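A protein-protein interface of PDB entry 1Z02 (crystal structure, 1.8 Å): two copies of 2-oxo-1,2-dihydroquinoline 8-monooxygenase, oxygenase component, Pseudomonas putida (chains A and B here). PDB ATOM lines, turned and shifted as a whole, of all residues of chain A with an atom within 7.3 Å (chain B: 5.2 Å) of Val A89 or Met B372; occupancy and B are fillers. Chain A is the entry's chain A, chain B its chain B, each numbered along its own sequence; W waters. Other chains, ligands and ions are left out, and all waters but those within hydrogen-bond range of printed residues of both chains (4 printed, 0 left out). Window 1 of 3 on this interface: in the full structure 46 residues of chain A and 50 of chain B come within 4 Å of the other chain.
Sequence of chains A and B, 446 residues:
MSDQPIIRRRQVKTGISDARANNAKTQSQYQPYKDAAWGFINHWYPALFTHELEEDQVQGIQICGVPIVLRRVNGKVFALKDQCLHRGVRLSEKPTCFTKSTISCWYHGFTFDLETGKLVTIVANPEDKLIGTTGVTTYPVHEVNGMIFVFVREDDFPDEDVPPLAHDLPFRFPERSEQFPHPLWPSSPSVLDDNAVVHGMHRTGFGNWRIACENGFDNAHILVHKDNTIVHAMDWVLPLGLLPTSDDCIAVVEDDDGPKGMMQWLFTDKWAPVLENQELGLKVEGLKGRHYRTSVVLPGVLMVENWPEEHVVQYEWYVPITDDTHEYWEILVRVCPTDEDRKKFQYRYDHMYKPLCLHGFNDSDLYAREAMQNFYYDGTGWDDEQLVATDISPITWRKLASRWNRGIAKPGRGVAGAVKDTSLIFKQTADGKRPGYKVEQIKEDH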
ATOM      1  N   LYS A  81      -1.193 -14.699  33.009  1.00  0.00           N
ATOM      2  CA  LYS A  81      -0.301 -13.573  33.227  1.00  0.00           C
ATOM      3  C   LYS A  81      -1.016 -12.323  32.743  1.00  0.00           C
ATOM      4  O   LYS A  81      -1.518 -12.284  31.622  1.00  0.00           O
ATOM      5  CB  LYS A  81       1.006 -13.740  32.460  1.00  0.00           C
ATOM      6  CG  LYS A  81       1.993 -12.625  32.751  1.00  0.00           C
ATOM      7  CD  LYS A  81       3.250 -12.768  31.901  1.00  0.00           C
ATOM      8  CE  LYS A  81       4.089 -13.976  32.312  1.00  0.00           C
ATOM      9  NZ  LYS A  81       5.354 -14.045  31.518  1.00  0.00           N
ATOM     10  N   ASP A  82      -1.061 -11.306  33.598  1.00  0.00           N
ATOM     11  CA  ASP A  82      -1.741 -10.052  33.284  1.00  0.00           C
ATOM     12  C   ASP A  82      -0.870  -9.191  32.369  1.00  0.00           C
ATOM     13  O   ASP A  82      -0.441  -8.089  32.748  1.00  0.00           O
ATOM     14  CB  ASP A  82      -2.049  -9.301  34.584  1.00  0.00           C
ATOM     15  CG  ASP A  82      -3.121  -8.238  34.411  1.00  0.00           C
ATOM     16  OD1 ASP A  82      -3.308  -7.448  35.357  1.00  0.00           O
ATOM     17  OD2 ASP A  82      -3.772  -8.203  33.337  1.00  0.00           O
ATOM     18  N   GLN A  83      -0.625  -9.691  31.161  1.00  0.00           N
ATOM     19  CA  GLN A  83       0.211  -8.987  30.182  1.00  0.00           C
ATOM     20  C   GLN A  83      -0.079  -9.470  28.766  1.00  0.00           C
ATOM     21  O   GLN A  83       0.210 -10.609  28.416  1.00  0.00           O
ATOM     22  CB  GLN A  83       1.697  -9.214  30.478  1.00  0.00           C
ATOM     23  CG  GLN A  83       2.635  -8.518  29.486  1.00  0.00           C
ATOM     24  CD  GLN A  83       4.065  -9.025  29.580  1.00  0.00           C
ATOM     25  OE1 GLN A  83       4.354 -10.184  29.250  1.00  0.00           O
ATOM     26  NE2 GLN A  83       4.969  -8.163  30.038  1.00  0.00           N
ATOM     27  N   CYS A  84      -0.656  -8.599  27.951  1.00  0.00           N
ATOM     28  CA  CYS A  84      -0.974  -8.948  26.576  1.00  0.00           C
ATOM     29  C   CYS A  84       0.329  -9.075  25.798  1.00  0.00           C
ATOM     30  O   CYS A  84       1.217  -8.232  25.954  1.00  0.00           O
ATOM     31  CB  CYS A  84      -1.847  -7.866  25.948  1.00  0.00           C
ATOM     32  SG  CYS A  84      -2.340  -8.267  24.253  1.00  0.00           S
ATOM     33  N   LEU A  85       0.425 -10.123  24.970  1.00  0.00           N
ATOM     34  CA  LEU A  85       1.606 -10.412  24.142  1.00  0.00           C
ATOM     35  C   LEU A  85       1.813  -9.384  23.068  1.00  0.00           C
ATOM     36  O   LEU A  85       2.923  -9.225  22.566  1.00  0.00           O
ATOM     37  CB  LEU A  85       1.462 -11.714  23.365  1.00  0.00           C
ATOM     38  CG  LEU A  85       0.825 -12.949  23.931  1.00  0.00           C
ATOM     39  CD1 LEU A  85       0.808 -14.081  22.916  1.00  0.00           C
ATOM     40  CD2 LEU A  85       1.588 -13.294  25.135  1.00  0.00           C
ATOM     41  N   HIS A  86       0.729  -8.743  22.654  1.00  0.00           N
ATOM     42  CA  HIS A  86       0.843  -7.761  21.603  1.00  0.00           C
ATOM     43  C   HIS A  86       1.702  -6.593  22.046  1.00  0.00           C
ATOM     44  O   HIS A  86       2.864  -6.497  21.652  1.00  0.00           O
ATOM     45  CB  HIS A  86      -0.526  -7.241  21.163  1.00  0.00           C
ATOM     46  CG  HIS A  86      -0.465  -6.406  19.922  1.00  0.00           C
ATOM     47  ND1 HIS A  86      -1.375  -5.404  19.643  1.00  0.00           N
ATOM     48  CD2 HIS A  86       0.404  -6.411  18.884  1.00  0.00           C
ATOM     49  CE1 HIS A  86      -1.066  -4.834  18.498  1.00  0.00           C
ATOM     50  NE2 HIS A  86       0.013  -5.426  18.013  1.00  0.00           N
ATOM     51  N   ARG A  87       1.135  -5.712  22.868  1.00  0.00           N
ATOM     52  CA  ARG A  87       1.871  -4.543  23.326  1.00  0.00           C
ATOM     53  C   ARG A  87       1.937  -4.321  24.839  1.00  0.00           C
ATOM     54  O   ARG A  87       2.013  -3.187  25.309  1.00  0.00           O
ATOM     55  CB  ARG A  87       1.349  -3.301  22.600  1.00  0.00           C
ATOM     56  CG  ARG A  87       1.405  -3.484  21.088  1.00  0.00           C
ATOM     57  CD  ARG A  87       1.254  -2.191  20.322  1.00  0.00           C
ATOM     58  NE  ARG A  87       2.372  -1.288  20.579  1.00  0.00           N
ATOM     59  CZ  ARG A  87       2.642  -0.211  19.853  1.00  0.00           C
ATOM     60  NH1 ARG A  87       3.677   0.551  20.170  1.00  0.00           N
ATOM     61  NH2 ARG A  87       1.885   0.098  18.812  1.00  0.00           N
ATOM     62  N   GLY A  88       1.907  -5.425  25.585  1.00  0.00           N
ATOM     63  CA  GLY A  88       2.073  -5.396  27.034  1.00  0.00           C
ATOM     64  C   GLY A  88       1.078  -4.763  27.979  1.00  0.00           C
ATOM     65  O   GLY A  88       1.411  -4.490  29.137  1.00  0.00           O
ATOM     66  N   VAL A  89      -0.128  -4.518  27.485  1.00  0.00           N
ATOM     67  CA  VAL A  89      -1.192  -3.945  28.283  1.00  0.00           C
ATOM     68  C   VAL A  89      -1.662  -4.970  29.305  1.00  0.00           C
ATOM     69  O   VAL A  89      -1.664  -6.178  29.040  1.00  0.00           O
ATOM     70  CB  VAL A  89      -2.387  -3.560  27.387  1.00  0.00           C
ATOM     71  CG1 VAL A  89      -3.592  -3.235  28.221  1.00  0.00           C
ATOM     72  CG2 VAL A  89      -2.020  -2.375  26.521  1.00  0.00           C
ATOM     73  N   ARG A  90      -2.052  -4.475  30.474  1.00  0.00           N
ATOM     74  CA  ARG A  90      -2.570  -5.307  31.554  1.00  0.00           C
ATOM     75  C   ARG A  90      -4.034  -5.607  31.212  1.00  0.00           C
ATOM     76  O   ARG A  90      -4.867  -4.693  31.149  1.00  0.00           O
ATOM     77  CB  ARG A  90      -2.473  -4.538  32.876  1.00  0.00           C
ATOM     78  CG  ARG A  90      -1.834  -5.325  33.996  1.00  0.00           C
ATOM     79  CD  ARG A  90      -1.147  -4.484  35.056  1.00  0.00           C
ATOM     80  NE  ARG A  90      -1.625  -3.112  35.172  1.00  0.00           N
ATOM     81  CZ  ARG A  90      -1.191  -2.264  36.103  1.00  0.00           C
ATOM     82  NH1 ARG A  90      -1.654  -1.016  36.155  1.00  0.00           N
ATOM     83  NH2 ARG A  90      -0.300  -2.669  36.999  1.00  0.00           N
ATOM     84  N   LEU A  91      -4.342  -6.879  30.981  1.00  0.00           N
ATOM     85  CA  LEU A  91      -5.694  -7.289  30.624  1.00  0.00           C
ATOM     86  C   LEU A  91      -6.747  -6.923  31.666  1.00  0.00           C
ATOM     87  O   LEU A  91      -7.879  -6.589  31.316  1.00  0.00           O
ATOM     88  CB  LEU A  91      -5.742  -8.805  30.384  1.00  0.00           C
ATOM     89  CG  LEU A  91      -4.707  -9.387  29.412  1.00  0.00           C
ATOM     90  CD1 LEU A  91      -4.801 -10.908  29.446  1.00  0.00           C
ATOM     91  CD2 LEU A  91      -4.949  -8.869  28.006  1.00  0.00           C
ATOM     92  N   SER A  92      -6.363  -6.980  32.939  1.00  0.00           N
ATOM     93  CA  SER A  92      -7.258  -6.693  34.052  1.00  0.00           C
ATOM     94  C   SER A  92      -7.702  -5.242  34.206  1.00  0.00           C
ATOM     95  O   SER A  92      -8.637  -4.974  34.940  1.00  0.00           O
ATOM     96  CB  SER A  92      -6.603  -7.138  35.367  1.00  0.00           C
ATOM     97  OG  SER A  92      -5.503  -6.309  35.691  1.00  0.00           O
ATOM     98  N   GLU A  93      -7.052  -4.306  33.527  1.00  0.00           N
ATOM     99  CA  GLU A  93      -7.428  -2.905  33.695  1.00  0.00           C
ATOM    100  C   GLU A  93      -8.830  -2.591  33.202  1.00  0.00           C
ATOM    101  O   GLU A  93      -9.488  -1.684  33.703  1.00  0.00           O
ATOM    102  CB  GLU A  93      -6.399  -2.002  33.013  1.00  0.00           C
ATOM    103  CG  GLU A  93      -5.135  -1.848  33.843  1.00  0.00           C
ATOM    104  CD  GLU A  93      -4.254  -0.724  33.379  1.00  0.00           C
ATOM    105  OE1 GLU A  93      -4.784   0.367  33.105  1.00  0.00           O
ATOM    106  OE2 GLU A  93      -3.030  -0.922  33.309  1.00  0.00           O
ATOM    107  N   LYS A  94      -9.287  -3.330  32.204  1.00  0.00           N
ATOM    108  CA  LYS A  94     -10.628  -3.131  31.678  1.00  0.00           C
ATOM    109  C   LYS A  94     -11.133  -4.500  31.242  1.00  0.00           C
ATOM    110  O   LYS A  94     -11.051  -4.864  30.073  1.00  0.00           O
ATOM    111  CB  LYS A  94     -10.605  -2.163  30.500  1.00  0.00           C
ATOM    112  CG  LYS A  94     -11.987  -1.709  30.142  1.00  0.00           C
ATOM    113  CD  LYS A  94     -12.019  -0.749  28.996  1.00  0.00           C
ATOM    114  CE  LYS A  94     -13.476  -0.408  28.727  1.00  0.00           C
ATOM    115  NZ  LYS A  94     -13.688   0.400  27.505  1.00  0.00           N
ATOM    116  N   CYS A 105      -7.894  -8.825  25.347  1.00  0.00           N
ATOM    117  CA  CYS A 105      -7.213  -7.598  25.697  1.00  0.00           C
ATOM    118  C   CYS A 105      -8.141  -6.503  25.199  1.00  0.00           C
ATOM    119  O   CYS A 105      -8.660  -6.585  24.081  1.00  0.00           O
ATOM    120  CB  CYS A 105      -5.866  -7.498  24.994  1.00  0.00           C
ATOM    121  SG  CYS A 105      -5.029  -5.931  25.312  1.00  0.00           S
ATOM    122  N   TRP A 106      -8.354  -5.493  26.036  1.00  0.00           N
ATOM    123  CA  TRP A 106      -9.241  -4.386  25.706  1.00  0.00           C
ATOM    124  C   TRP A 106      -8.689  -3.383  24.701  1.00  0.00           C
ATOM    125  O   TRP A 106      -9.365  -2.411  24.365  1.00  0.00           O
ATOM    126  CB  TRP A 106      -9.647  -3.632  26.977  1.00  0.00           C
ATOM    127  CG  TRP A 106      -8.493  -3.276  27.872  1.00  0.00           C
ATOM    128  CD1 TRP A 106      -7.896  -4.082  28.796  1.00  0.00           C
ATOM    129  CD2 TRP A 106      -7.814  -2.019  27.937  1.00  0.00           C
ATOM    130  NE1 TRP A 106      -6.888  -3.404  29.442  1.00  0.00           N
ATOM    131  CE2 TRP A 106      -6.821  -2.134  28.935  1.00  0.00           C
ATOM    132  CE3 TRP A 106      -7.955  -0.803  27.256  1.00  0.00           C
ATOM    133  CZ2 TRP A 106      -5.964  -1.073  29.260  1.00  0.00           C
ATOM    134  CZ3 TRP A 106      -7.099   0.252  27.583  1.00  0.00           C
ATOM    135  CH2 TRP A 106      -6.122   0.108  28.578  1.00  0.00           C
ATOM    136  N   TYR A 107      -7.471  -3.594  24.222  1.00  0.00           N
ATOM    137  CA  TYR A 107      -6.925  -2.658  23.257  1.00  0.00           C
ATOM    138  C   TYR A 107      -7.243  -3.112  21.833  1.00  0.00           C
ATOM    139  O   TYR A 107      -8.114  -2.535  21.191  1.00  0.00           O
ATOM    140  CB  TYR A 107      -5.415  -2.488  23.447  1.00  0.00           C
ATOM    141  CG  TYR A 107      -4.849  -1.261  22.757  1.00  0.00           C
ATOM    142  CD1 TYR A 107      -3.492  -0.957  22.829  1.00  0.00           C
ATOM    143  CD2 TYR A 107      -5.668  -0.416  22.015  1.00  0.00           C
ATOM    144  CE1 TYR A 107      -2.968   0.155  22.176  1.00  0.00           C
ATOM    145  CE2 TYR A 107      -5.156   0.689  21.364  1.00  0.00           C
ATOM    146  CZ  TYR A 107      -3.810   0.971  21.443  1.00  0.00           C
ATOM    147  OH  TYR A 107      -3.312   2.061  20.762  1.00  0.00           O
ATOM    148  N   HIS A 108      -6.559  -4.145  21.343  1.00  0.00           N
ATOM    149  CA  HIS A 108      -6.803  -4.620  19.981  1.00  0.00           C
ATOM    150  C   HIS A 108      -7.520  -5.964  19.916  1.00  0.00           C
ATOM    151  O   HIS A 108      -7.739  -6.499  18.832  1.00  0.00           O
ATOM    152  CB  HIS A 108      -5.493  -4.727  19.204  1.00  0.00           C
ATOM    153  CG  HIS A 108      -4.729  -3.445  19.122  1.00  0.00           C
ATOM    154  ND1 HIS A 108      -3.710  -3.124  19.993  1.00  0.00           N
ATOM    155  CD2 HIS A 108      -4.842  -2.395  18.277  1.00  0.00           C
ATOM    156  CE1 HIS A 108      -3.229  -1.933  19.688  1.00  0.00           C
ATOM    157  NE2 HIS A 108      -3.900  -1.468  18.650  1.00  0.00           N
ATOM    158  N   GLY A 414       9.613  -4.994  32.051  1.00  0.00           N
ATOM    159  CA  GLY A 414       8.503  -4.646  31.179  1.00  0.00           C
ATOM    160  C   GLY A 414       7.146  -4.805  31.839  1.00  0.00           C
ATOM    161  O   GLY A 414       6.145  -5.048  31.163  1.00  0.00           O
ATOM    162  N   LEU A 424       4.364   7.726  35.814  1.00  0.00           N
ATOM    163  CA  LEU A 424       3.059   7.169  36.172  1.00  0.00           C
ATOM    164  C   LEU A 424       2.970   6.995  37.685  1.00  0.00           C
ATOM    165  O   LEU A 424       1.931   7.280  38.295  1.00  0.00           O
ATOM    166  CB  LEU A 424       2.841   5.800  35.525  1.00  0.00           C
ATOM    167  CG  LEU A 424       2.270   5.791  34.105  1.00  0.00           C
ATOM    168  CD1 LEU A 424       2.303   4.366  33.550  1.00  0.00           C
ATOM    169  CD2 LEU A 424       0.850   6.347  34.132  1.00  0.00           C
ATOM    170  N   ILE B 211       4.706   5.944  22.230  1.00  0.00           N
ATOM    171  CA  ILE B 211       3.567   5.101  22.564  1.00  0.00           C
ATOM    172  C   ILE B 211       2.256   5.832  22.349  1.00  0.00           C
ATOM    173  O   ILE B 211       1.271   5.243  21.914  1.00  0.00           O
ATOM    174  CB  ILE B 211       3.649   4.653  24.040  1.00  0.00           C
ATOM    175  CG1 ILE B 211       4.888   3.776  24.234  1.00  0.00           C
ATOM    176  CG2 ILE B 211       2.385   3.934  24.455  1.00  0.00           C
ATOM    177  CD1 ILE B 211       5.026   2.620  23.217  1.00  0.00           C
ATOM    178  N   ALA B 368      -5.516   3.931  27.326  1.00  0.00           N
ATOM    179  CA  ALA B 368      -4.893   2.906  26.505  1.00  0.00           C
ATOM    180  C   ALA B 368      -3.388   3.151  26.459  1.00  0.00           C
ATOM    181  O   ALA B 368      -2.592   2.231  26.625  1.00  0.00           O
ATOM    182  CB  ALA B 368      -5.474   2.930  25.100  1.00  0.00           C
ATOM    183  N   ARG B 369      -3.005   4.404  26.245  1.00  0.00           N
ATOM    184  CA  ARG B 369      -1.601   4.772  26.171  1.00  0.00           C
ATOM    185  C   ARG B 369      -0.855   4.498  27.469  1.00  0.00           C
ATOM    186  O   ARG B 369       0.222   3.907  27.458  1.00  0.00           O
ATOM    187  CB  ARG B 369      -1.481   6.256  25.807  1.00  0.00           C
ATOM    188  CG  ARG B 369      -2.070   6.577  24.452  1.00  0.00           C
ATOM    189  CD  ARG B 369      -2.207   8.066  24.260  1.00  0.00           C
ATOM    190  NE  ARG B 369      -2.941   8.368  23.041  1.00  0.00           N
ATOM    191  CZ  ARG B 369      -3.271   9.593  22.652  1.00  0.00           C
ATOM    192  NH1 ARG B 369      -3.946   9.775  21.525  1.00  0.00           N
ATOM    193  NH2 ARG B 369      -2.923  10.637  23.390  1.00  0.00           N
ATOM    194  N   GLU B 370      -1.431   4.921  28.589  1.00  0.00           N
ATOM    195  CA  GLU B 370      -0.788   4.722  29.873  1.00  0.00           C
ATOM    196  C   GLU B 370      -0.592   3.250  30.157  1.00  0.00           C
ATOM    197  O   GLU B 370       0.452   2.856  30.664  1.00  0.00           O
ATOM    198  CB  GLU B 370      -1.605   5.366  31.000  1.00  0.00           C
ATOM    199  CG  GLU B 370      -1.429   6.882  31.116  1.00  0.00           C
ATOM    200  CD  GLU B 370      -2.206   7.488  32.280  1.00  0.00           C
ATOM    201  OE1 GLU B 370      -2.703   6.717  33.129  1.00  0.00           O
ATOM    202  OE2 GLU B 370      -2.310   8.738  32.352  1.00  0.00           O
ATOM    203  N   ALA B 371      -1.592   2.440  29.814  1.00  0.00           N
ATOM    204  CA  ALA B 371      -1.535   1.002  30.050  1.00  0.00           C
ATOM    205  C   ALA B 371      -0.361   0.303  29.360  1.00  0.00           C
ATOM    206  O   ALA B 371       0.111  -0.732  29.833  1.00  0.00           O
ATOM    207  CB  ALA B 371      -2.859   0.356  29.625  1.00  0.00           C
ATOM    208  N   MET B 372       0.111   0.867  28.254  1.00  0.00           N
ATOM    209  CA  MET B 372       1.227   0.293  27.490  1.00  0.00           C
ATOM    210  C   MET B 372       2.627   0.672  27.972  1.00  0.00           C
ATOM    211  O   MET B 372       3.579  -0.083  27.803  1.00  0.00           O
ATOM    212  CB  MET B 372       1.123   0.711  26.021  1.00  0.00           C
ATOM    213  CG  MET B 372       0.407  -0.277  25.121  1.00  0.00           C
ATOM    214  SD  MET B 372       0.214   0.368  23.442  1.00  0.00           S
ATOM    215  CE  MET B 372       1.716   0.988  23.126  1.00  0.00           C
ATOM    216  N   GLN B 373       2.752   1.849  28.564  1.00  0.00           N
ATOM    217  CA  GLN B 373       4.058   2.354  28.983  1.00  0.00           C
ATOM    218  C   GLN B 373       5.022   1.427  29.756  1.00  0.00           C
ATOM    219  O   GLN B 373       6.204   1.343  29.410  1.00  0.00           O
ATOM    220  CB  GLN B 373       3.851   3.677  29.726  1.00  0.00           C
ATOM    221  CG  GLN B 373       2.980   4.680  28.936  1.00  0.00           C
ATOM    222  CD  GLN B 373       3.679   5.286  27.717  1.00  0.00           C
ATOM    223  OE1 GLN B 373       4.748   4.850  27.310  1.00  0.00           O
ATOM    224  NE2 GLN B 373       3.063   6.301  27.131  1.00  0.00           N
ATOM    225  N   ASN B 374       4.540   0.735  30.785  1.00  0.00           N
ATOM    226  CA  ASN B 374       5.398  -0.164  31.573  1.00  0.00           C
ATOM    227  C   ASN B 374       6.122  -1.239  30.748  1.00  0.00           C
ATOM    228  O   ASN B 374       7.256  -1.609  31.054  1.00  0.00           O
ATOM    229  CB  ASN B 374       4.581  -0.854  32.670  1.00  0.00           C
ATOM    230  CG  ASN B 374       4.205   0.083  33.800  1.00  0.00           C
ATOM    231  OD1 ASN B 374       3.355  -0.243  34.631  1.00  0.00           O
ATOM    232  ND2 ASN B 374       4.842   1.246  33.847  1.00  0.00           N
ATOM    233  N   PHE B 375       5.463  -1.752  29.713  1.00  0.00           N
ATOM    234  CA  PHE B 375       6.056  -2.788  28.868  1.00  0.00           C
ATOM    235  C   PHE B 375       7.262  -2.243  28.114  1.00  0.00           C
ATOM    236  O   PHE B 375       8.238  -2.957  27.878  1.00  0.00           O
ATOM    237  CB  PHE B 375       5.000  -3.292  27.871  1.00  0.00           C
ATOM    238  CG  PHE B 375       5.429  -4.480  27.042  1.00  0.00           C
ATOM    239  CD1 PHE B 375       5.969  -5.610  27.645  1.00  0.00           C
ATOM    240  CD2 PHE B 375       5.214  -4.499  25.664  1.00  0.00           C
ATOM    241  CE1 PHE B 375       6.284  -6.739  26.895  1.00  0.00           C
ATOM    242  CE2 PHE B 375       5.526  -5.625  24.898  1.00  0.00           C
ATOM    243  CZ  PHE B 375       6.061  -6.752  25.520  1.00  0.00           C
ATOM    244  N   TYR B 376       7.200  -0.959  27.780  1.00  0.00           N
ATOM    245  CA  TYR B 376       8.231  -0.298  26.981  1.00  0.00           C
ATOM    246  C   TYR B 376       9.326   0.546  27.621  1.00  0.00           C
ATOM    247  O   TYR B 376      10.437   0.601  27.092  1.00  0.00           O
ATOM    248  CB  TYR B 376       7.544   0.586  25.943  1.00  0.00           C
ATOM    249  CG  TYR B 376       6.781  -0.172  24.903  1.00  0.00           C
ATOM    250  CD1 TYR B 376       7.387  -0.539  23.703  1.00  0.00           C
ATOM    251  CD2 TYR B 376       5.445  -0.521  25.109  1.00  0.00           C
ATOM    252  CE1 TYR B 376       6.687  -1.225  22.727  1.00  0.00           C
ATOM    253  CE2 TYR B 376       4.736  -1.213  24.141  1.00  0.00           C
ATOM    254  CZ  TYR B 376       5.367  -1.562  22.954  1.00  0.00           C
ATOM    255  OH  TYR B 376       4.692  -2.273  21.995  1.00  0.00           O
HETATM  256  O   HOH W   1       2.261  -2.073  30.717  1.00  0.00           O
HETATM  257  O   HOH W   2      -1.234  -2.017  31.785  1.00  0.00           O
HETATM  258  O   HOH W   3       1.293   2.706  20.918  1.00  0.00           O
HETATM  259  O   HOH W   4       0.365   0.465  34.064  1.00  0.00           O
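Val A89 touches just these residues of chain B: Ala B371 (3.8 Å) and Met B372 (3.5 Å). Of the printed residues of chain A, Asn B374 touches Gly A414 (3.3 Å). Of the printed residues of chain A, Phe B375 touches Gln A83 (3.6 Å), Arg A87 (3.4 Å), Gly A88 (3.4 Å) and Gly A414 (3.2 Å). Printed residues of chain B within 4 Å of Trp A106: Ala B368 and Ala B371. Of the printed residues of chain B, Gly A414 touches Asn B374 and Phe B375. Cys A84 touches none of the printed residues of chain B. The nearest residue of chain A that does not touch Met B372 is Gly A88 (5.1 Å).
Of the 10 printed residues of chain B, 8 touch a printed residue of chain A. Of the 20 printed residues of chain A, 9 touch a printed residue of chain B. Hydrophobic or aromatic side chains of chain A within 4 Å of the printed part of chain B: Val A89, Trp A106, Tyr A107 and Leu A424. Among the printed residues, no Asp or Glu carboxylate lies within 4 Å of a Lys or Arg side-chain nitrogen of the other chain.
No position is printed for both chains.
The backbone NH (N) of Cys A84 is in hydrogen-bond range of the backbone carbonyl oxygen (O) of Val A89 (2.8 Å). NH1 of Arg A90 lies within salt-bridge range of OE2 of Glu A93 (3.2 Å). The backbone carbonyl oxygen of Arg A90 lies within hydrogen-bond range of the indole nitrogen of Trp A106. SG of Cys A105 lies close to N of Tyr A107, 3.6 Å away.
The guanidinium group (NE) of Arg A87 lies within hydrogen-bond range of the side-chain hydroxyl (OH) of Tyr B376, 2.9 Å away.
Gln A83 touches Phe B375. Arg A87 touches Ile B211 (NH1 to CD1, 3.9 Å). CG of Met B372 touches O of Arg A87, at 3.3 Å. Phe B375 touches Gly A88 (CD2 to N, 3.4 Å). Met B372 touches Val A89. CB of Ala B371 touches OE2 of Glu A93, at 3.9 Å. Trp A106 touches Ala B371 (CH2 to CB, 3.4 Å). Tyr A107 touches Met B372 (CE1 to SD, 3.4 Å). O of Asn B374 touches CA of Gly A414, at 3.3 Å. CD2 of Leu A424 touches OE1 of Glu B370, 3.7 Å away.
Water W2 lies within hydrogen-bond range of the side-chain carboxylate (OE2) of Glu A93 (2.6 Å), the backbone carbonyl oxygen (O) of Ala B371 (2.7 Å) and the backbone NH (N) of Arg A90 (2.9 Å). Water W1 lies within hydrogen-bond range of O of Ala B371, O of Gly A88 and N of Phe B375. Water W3 lies within hydrogen-bond range of O of Ile B211, NH1 of Arg A87 and SD of Met B372. Water W4 lies within hydrogen-bond range of the side-chain amide oxygen (OD1) of Asn B374 and the guanidinium group (NH1) of Arg A90.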
